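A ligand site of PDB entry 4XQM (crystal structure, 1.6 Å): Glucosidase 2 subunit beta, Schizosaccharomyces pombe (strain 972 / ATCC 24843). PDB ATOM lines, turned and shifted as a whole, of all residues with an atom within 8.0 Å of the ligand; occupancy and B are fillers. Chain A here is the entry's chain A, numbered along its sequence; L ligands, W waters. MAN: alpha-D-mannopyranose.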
ATOM      1  N   TYR A  16       3.500  20.165 -22.467  1.00  0.00           N
ATOM      2  CA  TYR A  16       2.827  21.131 -23.340  1.00  0.00           C
ATOM      3  C   TYR A  16       3.816  21.997 -24.088  1.00  0.00           C
ATOM      4  O   TYR A  16       4.810  22.460 -23.514  1.00  0.00           O
ATOM      5  CB  TYR A  16       1.955  22.095 -22.537  1.00  0.00           C
ATOM      6  CG  TYR A  16       0.935  21.490 -21.607  1.00  0.00           C
ATOM      7  CD1 TYR A  16      -0.235  20.920 -22.093  1.00  0.00           C
ATOM      8  CD2 TYR A  16       1.116  21.536 -20.232  1.00  0.00           C
ATOM      9  CE1 TYR A  16      -1.187  20.409 -21.231  1.00  0.00           C
ATOM     10  CE2 TYR A  16       0.165  21.024 -19.361  1.00  0.00           C
ATOM     11  CZ  TYR A  16      -0.977  20.456 -19.862  1.00  0.00           C
ATOM     12  OH  TYR A  16      -1.908  19.944 -18.994  1.00  0.00           O
ATOM     13  N   TYR A  18       4.110  25.527 -25.094  1.00  0.00           N
ATOM     14  CA  TYR A  18       3.530  26.858 -24.937  1.00  0.00           C
ATOM     15  C   TYR A  18       4.092  27.770 -26.010  1.00  0.00           C
ATOM     16  O   TYR A  18       5.293  27.750 -26.284  1.00  0.00           O
ATOM     17  CB  TYR A  18       3.829  27.405 -23.547  1.00  0.00           C
ATOM     18  CG  TYR A  18       2.991  26.782 -22.458  1.00  0.00           C
ATOM     19  CD1 TYR A  18       1.687  27.224 -22.214  1.00  0.00           C
ATOM     20  CD2 TYR A  18       3.489  25.759 -21.658  1.00  0.00           C
ATOM     21  CE1 TYR A  18       0.904  26.636 -21.214  1.00  0.00           C
ATOM     22  CE2 TYR A  18       2.726  25.181 -20.651  1.00  0.00           C
ATOM     23  CZ  TYR A  18       1.439  25.624 -20.430  1.00  0.00           C
ATOM     24  OH  TYR A  18       0.674  25.056 -19.433  1.00  0.00           O
ATOM     25  N   GLN A  28      -1.405  26.570 -25.913  1.00  0.00           N
ATOM     26  CA  GLN A  28      -0.855  25.450 -25.168  1.00  0.00           C
ATOM     27  C   GLN A  28      -1.150  24.234 -26.034  1.00  0.00           C
ATOM     28  O   GLN A  28      -2.316  23.835 -26.155  1.00  0.00           O
ATOM     29  CB  GLN A  28      -1.593  25.315 -23.827  1.00  0.00           C
ATOM     30  CG  GLN A  28      -1.174  24.118 -22.971  1.00  0.00           C
ATOM     31  CD  GLN A  28      -2.207  23.797 -21.921  1.00  0.00           C
ATOM     32  OE1 GLN A  28      -3.332  23.420 -22.263  1.00  0.00           O
ATOM     33  NE2 GLN A  28      -1.832  23.940 -20.649  1.00  0.00           N
ATOM     34  N   ASP A  29      -0.105  23.661 -26.645  1.00  0.00           N
ATOM     35  CA  ASP A  29      -0.297  22.719 -27.759  1.00  0.00           C
ATOM     36  C   ASP A  29      -1.253  23.370 -28.760  1.00  0.00           C
ATOM     37  O   ASP A  29      -1.018  24.504 -29.160  1.00  0.00           O
ATOM     38  CB  ASP A  29      -0.765  21.348 -27.257  1.00  0.00           C
ATOM     39  CG  ASP A  29       0.310  20.637 -26.445  1.00  0.00           C
ATOM     40  OD1 ASP A  29       1.506  20.888 -26.724  1.00  0.00           O
ATOM     41  OD2 ASP A  29      -0.040  19.826 -25.538  1.00  0.00           O
ATOM     42  N   ILE A  31      -4.381  24.233 -28.115  1.00  0.00           N
ATOM     43  CA  ILE A  31      -5.437  24.921 -27.394  1.00  0.00           C
ATOM     44  C   ILE A  31      -5.187  26.429 -27.299  1.00  0.00           C
ATOM     45  O   ILE A  31      -4.094  26.863 -26.907  1.00  0.00           O
ATOM     46  CB  ILE A  31      -5.582  24.332 -25.963  1.00  0.00           C
ATOM     47  CG1 ILE A  31      -5.827  22.822 -26.029  1.00  0.00           C
ATOM     48  CG2 ILE A  31      -6.716  25.038 -25.216  1.00  0.00           C
ATOM     49  CD1 ILE A  31      -5.838  22.156 -24.647  1.00  0.00           C
ATOM     50  N   LEU A  32      -6.184  27.237 -27.682  1.00  0.00           N
ATOM     51  CA  LEU A  32      -6.066  28.691 -27.535  1.00  0.00           C
ATOM     52  C   LEU A  32      -6.209  29.092 -26.071  1.00  0.00           C
ATOM     53  O   LEU A  32      -7.237  28.833 -25.437  1.00  0.00           O
ATOM     54  CB  LEU A  32      -7.134  29.423 -28.367  1.00  0.00           C
ATOM     55  CG  LEU A  32      -7.156  30.956 -28.200  1.00  0.00           C
ATOM     56  CD1 LEU A  32      -5.913  31.585 -28.804  1.00  0.00           C
ATOM     57  CD2 LEU A  32      -8.403  31.537 -28.855  1.00  0.00           C
ATOM     58  N   LEU A  33      -5.164  29.739 -25.538  1.00  0.00           N
ATOM     59  CA  LEU A  33      -5.225  30.275 -24.174  1.00  0.00           C
ATOM     60  C   LEU A  33      -5.837  31.672 -24.129  1.00  0.00           C
ATOM     61  O   LEU A  33      -6.377  32.086 -23.111  1.00  0.00           O
ATOM     62  CB  LEU A  33      -3.828  30.297 -23.545  1.00  0.00           C
ATOM     63  CG  LEU A  33      -3.510  29.117 -22.628  1.00  0.00           C
ATOM     64  CD1 LEU A  33      -4.065  27.791 -23.146  1.00  0.00           C
ATOM     65  CD2 LEU A  33      -2.016  29.016 -22.309  1.00  0.00           C
ATOM     66  N   GLN A  50     -10.046  29.005 -25.326  1.00  0.00           N
ATOM     67  CA  GLN A  50     -10.917  27.847 -25.451  1.00  0.00           C
ATOM     68  C   GLN A  50     -11.605  27.492 -24.130  1.00  0.00           C
ATOM     69  O   GLN A  50     -11.061  27.726 -23.037  1.00  0.00           O
ATOM     70  CB  GLN A  50     -10.119  26.636 -25.958  1.00  0.00           C
ATOM     71  CG  GLN A  50     -10.954  25.359 -26.116  1.00  0.00           C
ATOM     72  CD  GLN A  50     -10.146  24.168 -26.625  1.00  0.00           C
ATOM     73  OE1 GLN A  50     -10.046  23.130 -25.945  1.00  0.00           O
ATOM     74  NE2 GLN A  50      -9.596  24.286 -27.830  1.00  0.00           N
ATOM     75  N   SER A  51     -12.817  26.932 -24.242  1.00  0.00           N
ATOM     76  CA  SER A  51     -13.554  26.436 -23.093  1.00  0.00           C
ATOM     77  C   SER A  51     -12.758  25.387 -22.329  1.00  0.00           C
ATOM     78  O   SER A  51     -11.853  24.729 -22.878  1.00  0.00           O
ATOM     79  CB  SER A  51     -14.907  25.873 -23.525  1.00  0.00           C
ATOM     80  OG  SER A  51     -14.740  24.715 -24.310  1.00  0.00           O
ATOM     81  N   CYS A  52     -13.079  25.256 -21.044  1.00  0.00           N
ATOM     82  CA  CYS A  52     -12.324  24.456 -20.096  1.00  0.00           C
ATOM     83  C   CYS A  52     -13.285  23.635 -19.250  1.00  0.00           C
ATOM     84  O   CYS A  52     -14.181  24.188 -18.606  1.00  0.00           O
ATOM     85  CB  CYS A  52     -11.512  25.403 -19.208  1.00  0.00           C
ATOM     86  SG  CYS A  52     -10.539  24.636 -17.901  1.00  0.00           S
ATOM     87  N   TRP A  53     -13.114  22.324 -19.249  1.00  0.00           N
ATOM     88  CA  TRP A  53     -13.964  21.437 -18.467  1.00  0.00           C
ATOM     89  C   TRP A  53     -13.965  21.869 -17.008  1.00  0.00           C
ATOM     90  O   TRP A  53     -12.910  21.878 -16.357  1.00  0.00           O
ATOM     91  CB  TRP A  53     -13.442  20.012 -18.558  1.00  0.00           C
ATOM     92  CG  TRP A  53     -14.377  18.951 -18.086  1.00  0.00           C
ATOM     93  CD1 TRP A  53     -15.713  19.081 -17.821  1.00  0.00           C
ATOM     94  CD2 TRP A  53     -14.043  17.586 -17.813  1.00  0.00           C
ATOM     95  NE1 TRP A  53     -16.227  17.864 -17.394  1.00  0.00           N
ATOM     96  CE2 TRP A  53     -15.216  16.927 -17.387  1.00  0.00           C
ATOM     97  CE3 TRP A  53     -12.848  16.844 -17.900  1.00  0.00           C
ATOM     98  CZ2 TRP A  53     -15.238  15.587 -17.057  1.00  0.00           C
ATOM     99  CZ3 TRP A  53     -12.870  15.514 -17.570  1.00  0.00           C
ATOM    100  CH2 TRP A  53     -14.065  14.886 -17.148  1.00  0.00           C
ATOM    101  N   ASN A  54     -15.147  22.237 -16.495  1.00  0.00           N
ATOM    102  CA  ASN A  54     -15.323  22.631 -15.097  1.00  0.00           C
ATOM    103  C   ASN A  54     -14.560  23.896 -14.723  1.00  0.00           C
ATOM    104  O   ASN A  54     -14.316  24.163 -13.542  1.00  0.00           O
ATOM    105  CB  ASN A  54     -14.970  21.470 -14.155  1.00  0.00           C
ATOM    106  CG  ASN A  54     -15.999  20.366 -14.197  1.00  0.00           C
ATOM    107  OD1 ASN A  54     -17.193  20.637 -14.308  1.00  0.00           O
ATOM    108  ND2 ASN A  54     -15.541  19.112 -14.124  1.00  0.00           N
ATOM    109  N   GLY A  55     -14.238  24.703 -15.727  1.00  0.00           N
ATOM    110  CA  GLY A  55     -13.478  25.915 -15.487  1.00  0.00           C
ATOM    111  C   GLY A  55     -13.920  27.062 -16.363  1.00  0.00           C
ATOM    112  O   GLY A  55     -14.893  26.949 -17.126  1.00  0.00           O
ATOM    113  N   PRO A  56     -13.200  28.182 -16.283  1.00  0.00           N
ATOM    114  CA  PRO A  56     -13.509  29.357 -17.100  1.00  0.00           C
ATOM    115  C   PRO A  56     -12.929  29.184 -18.490  1.00  0.00           C
ATOM    116  O   PRO A  56     -11.980  28.415 -18.645  1.00  0.00           O
ATOM    117  CB  PRO A  56     -12.741  30.473 -16.378  1.00  0.00           C
ATOM    118  CG  PRO A  56     -11.533  29.764 -15.784  1.00  0.00           C
ATOM    119  CD  PRO A  56     -12.094  28.426 -15.344  1.00  0.00           C
ATOM    120  N   ARG A  58     -10.382  29.961 -21.170  1.00  0.00           N
ATOM    121  CA  ARG A  58      -8.996  30.207 -20.802  1.00  0.00           C
ATOM    122  C   ARG A  58      -8.573  31.671 -20.985  1.00  0.00           C
ATOM    123  O   ARG A  58      -9.150  32.403 -21.797  1.00  0.00           O
ATOM    124  CB  ARG A  58      -8.052  29.250 -21.547  1.00  0.00           C
ATOM    125  CG  ARG A  58      -8.197  27.774 -21.120  1.00  0.00           C
ATOM    126  CD  ARG A  58      -7.372  26.865 -22.014  1.00  0.00           C
ATOM    127  NE  ARG A  58      -7.432  25.451 -21.620  1.00  0.00           N
ATOM    128  CZ  ARG A  58      -8.470  24.671 -21.907  1.00  0.00           C
ATOM    129  NH1 ARG A  58      -9.492  25.192 -22.556  1.00  0.00           N
ATOM    130  NH2 ARG A  58      -8.489  23.390 -21.555  1.00  0.00           N
ATOM    131  N   VAL A  75       5.398  29.173 -16.492  1.00  0.00           N
ATOM    132  CA  VAL A  75       3.952  29.183 -16.611  1.00  0.00           C
ATOM    133  C   VAL A  75       3.356  28.680 -15.306  1.00  0.00           C
ATOM    134  O   VAL A  75       3.735  27.603 -14.822  1.00  0.00           O
ATOM    135  CB  VAL A  75       3.467  28.283 -17.771  1.00  0.00           C
ATOM    136  CG1 VAL A  75       1.933  28.206 -17.767  1.00  0.00           C
ATOM    137  CG2 VAL A  75       3.975  28.798 -19.111  1.00  0.00           C
ATOM    138  N   GLU A  77      -0.322  27.831 -13.419  1.00  0.00           N
ATOM    139  CA  GLU A  77      -1.769  27.679 -13.505  1.00  0.00           C
ATOM    140  C   GLU A  77      -2.266  27.460 -12.081  1.00  0.00           C
ATOM    141  O   GLU A  77      -2.662  26.367 -11.720  1.00  0.00           O
ATOM    142  CB  GLU A  77      -2.164  26.515 -14.411  1.00  0.00           C
ATOM    143  CG  GLU A  77      -3.661  26.464 -14.707  1.00  0.00           C
ATOM    144  CD  GLU A  77      -4.063  25.322 -15.651  1.00  0.00           C
ATOM    145  OE1 GLU A  77      -3.184  24.561 -16.129  1.00  0.00           O
ATOM    146  OE2 GLU A  77      -5.281  25.201 -15.921  1.00  0.00           O
ATOM    147  N   GLN A  79      -4.950  28.873 -10.643  1.00  0.00           N
ATOM    148  CA  GLN A  79      -6.384  28.600 -10.719  1.00  0.00           C
ATOM    149  C   GLN A  79      -6.631  27.921 -12.054  1.00  0.00           C
ATOM    150  O   GLN A  79      -5.993  28.267 -13.039  1.00  0.00           O
ATOM    151  CB  GLN A  79      -7.202  29.905 -10.640  1.00  0.00           C
ATOM    152  CG  GLN A  79      -7.224  30.562  -9.277  1.00  0.00           C
ATOM    153  CD  GLN A  79      -5.885  31.156  -8.862  1.00  0.00           C
ATOM    154  OE1 GLN A  79      -5.401  32.112  -9.471  1.00  0.00           O
ATOM    155  NE2 GLN A  79      -5.271  30.572  -7.836  1.00  0.00           N
ATOM    156  N   LYS A  80      -7.547  26.957 -12.078  1.00  0.00           N
ATOM    157  CA  LYS A  80      -7.822  26.190 -13.300  1.00  0.00           C
ATOM    158  C   LYS A  80      -8.105  27.095 -14.493  1.00  0.00           C
ATOM    159  O   LYS A  80      -8.972  27.990 -14.438  1.00  0.00           O
ATOM    160  CB  LYS A  80      -8.999  25.222 -13.084  1.00  0.00           C
ATOM    161  CG  LYS A  80      -9.303  24.366 -14.305  1.00  0.00           C
ATOM    162  CD  LYS A  80     -10.610  23.569 -14.116  1.00  0.00           C
ATOM    163  CE  LYS A  80     -10.516  22.576 -12.965  1.00  0.00           C
ATOM    164  NZ  LYS A  80      -9.687  21.356 -13.305  1.00  0.00           N
ATOM    165  N   CYS A  81      -7.322  26.896 -15.555  1.00  0.00           N
ATOM    166  CA  CYS A  81      -7.466  27.585 -16.836  1.00  0.00           C
ATOM    167  C   CYS A  81      -7.236  29.096 -16.798  1.00  0.00           C
ATOM    168  O   CYS A  81      -7.675  29.834 -17.685  1.00  0.00           O
ATOM    169  CB  CYS A  81      -8.784  27.195 -17.509  1.00  0.00           C
ATOM    170  SG  CYS A  81      -8.699  25.496 -18.114  1.00  0.00           S
ATOM    171  N   GLU A  82      -6.514  29.534 -15.767  1.00  0.00           N
ATOM    172  CA  GLU A  82      -6.002  30.895 -15.698  1.00  0.00           C
ATOM    173  C   GLU A  82      -4.476  30.768 -15.650  1.00  0.00           C
ATOM    174  O   GLU A  82      -3.925  30.218 -14.692  1.00  0.00           O
ATOM    175  CB  GLU A  82      -6.541  31.595 -14.430  1.00  0.00           C
ATOM    176  CG  GLU A  82      -8.073  31.611 -14.299  1.00  0.00           C
ATOM    177  CD  GLU A  82      -8.548  32.208 -12.967  1.00  0.00           C
ATOM    178  OE1 GLU A  82      -7.822  33.051 -12.384  1.00  0.00           O
ATOM    179  OE2 GLU A  82      -9.658  31.838 -12.507  1.00  0.00           O
ATOM    180  N   TYR A  83      -3.799  31.248 -16.687  1.00  0.00           N
ATOM    181  CA  TYR A  83      -2.376  31.021 -16.820  1.00  0.00           C
ATOM    182  C   TYR A  83      -1.592  32.301 -16.550  1.00  0.00           C
ATOM    183  O   TYR A  83      -1.913  33.362 -17.106  1.00  0.00           O
ATOM    184  CB  TYR A  83      -2.057  30.497 -18.220  1.00  0.00           C
ATOM    185  CG  TYR A  83      -2.844  29.250 -18.559  1.00  0.00           C
ATOM    186  CD1 TYR A  83      -4.157  29.342 -19.054  1.00  0.00           C
ATOM    187  CD2 TYR A  83      -2.303  27.990 -18.370  1.00  0.00           C
ATOM    188  CE1 TYR A  83      -4.888  28.203 -19.357  1.00  0.00           C
ATOM    189  CE2 TYR A  83      -3.033  26.842 -18.663  1.00  0.00           C
ATOM    190  CZ  TYR A  83      -4.324  26.953 -19.151  1.00  0.00           C
ATOM    191  OH  TYR A  83      -5.055  25.824 -19.453  1.00  0.00           O
HETATM  192  C1  MAN L   1      -5.686  20.960 -20.105  1.00  0.00           C
HETATM  193  C2  MAN L   1      -4.847  22.092 -20.047  1.00  0.00           C
HETATM  194  C3  MAN L   1      -4.753  22.463 -18.568  1.00  0.00           C
HETATM  195  C4  MAN L   1      -6.187  22.593 -17.950  1.00  0.00           C
HETATM  196  C5  MAN L   1      -6.950  21.270 -18.164  1.00  0.00           C
HETATM  197  C6  MAN L   1      -8.402  21.352 -17.759  1.00  0.00           C
HETATM  198  O1  MAN L   1      -4.909  20.156 -19.263  1.00  0.00           O
HETATM  199  O2  MAN L   1      -5.450  23.109 -20.757  1.00  0.00           O
HETATM  200  O3  MAN L   1      -3.995  23.628 -18.391  1.00  0.00           O
HETATM  201  O4  MAN L   1      -6.098  22.829 -16.568  1.00  0.00           O
HETATM  202  O5  MAN L   1      -6.938  21.015 -19.555  1.00  0.00           O
HETATM  203  O6  MAN L   1      -8.912  20.015 -17.706  1.00  0.00           O
HETATM  204  O   HOH W   1      -6.964  21.305 -14.372  1.00  0.00           O
HETATM  205  O   HOH W   2      -9.625  19.059 -20.272  1.00  0.00           O
HETATM  206  O   HOH W   3     -11.009  20.058 -15.890  1.00  0.00           O
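O3 of the ligand lies within hydrogen-bond range of OE1 of Glu 77, 2.6 Å away. An oxygen (O2) of the ligand is in hydrogen-bond range of the side-chain amide oxygen (OE1) of Gln 28 (2.6 Å). The side-chain hydroxyl (OH) of Tyr 83 is in hydrogen-bond range of an oxygen (O3) of the ligand. O1 of the ligand is in hydrogen-bond range of OH of Tyr 16 (3.0 Å). NH2 of Arg 58 lies within hydrogen-bond range of O2 of the ligand, 3.2 Å away.
The side-chain carboxylate (OE2) of Glu 77 sits at hydrogen-bond distance from the backbone NH (N) of Cys 81 (2.7 Å). The side-chain amide nitrogen (NE2) of Gln 28 is in hydrogen-bond range of the side-chain hydroxyl (OH) of Tyr 18, 3.0 Å away. The side-chain hydroxyl (OH) of Tyr 83 is in hydrogen-bond range of the guanidinium group (NE) of Arg 58, at 3.2 Å. The guanidinium group of Arg 58 is in hydrogen-bond range of the side-chain sulfur of Cys 81. The backbone NH of Arg 58 lies within hydrogen-bond range of the backbone carbonyl oxygen of Gln 50 (3.0 Å). The guanidinium group (NH1) of Arg 58 sits at hydrogen-bond distance from the backbone carbonyl oxygen (O) of Ser 51 (2.4 Å). The side-chain sulfur (SG) of Cys 81 is disulfide-bonded to the side-chain sulfur (SG) of Cys 52 (2.0 Å).
Merely in contact with the ligand: Cys 81 (3.8 Å) and Cys 52 (3.9 Å). Hydrophobic or aromatic side chains that line the ligand: Tyr 16 and Tyr 83. The nearest printed residue that does not touch the ligand is Ile 31 (4.02 Å).
Water W3 lies within hydrogen-bond range of the backbone carbonyl oxygen of Trp 53 (2.7 Å), an oxygen (O6) of the ligand (2.8 Å) and the side-chain amino group of Lys 80 (3.2 Å). Water W1 lies within hydrogen-bond range of O4 of the ligand (2.8 Å) and NZ of Lys 80 (2.9 Å).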
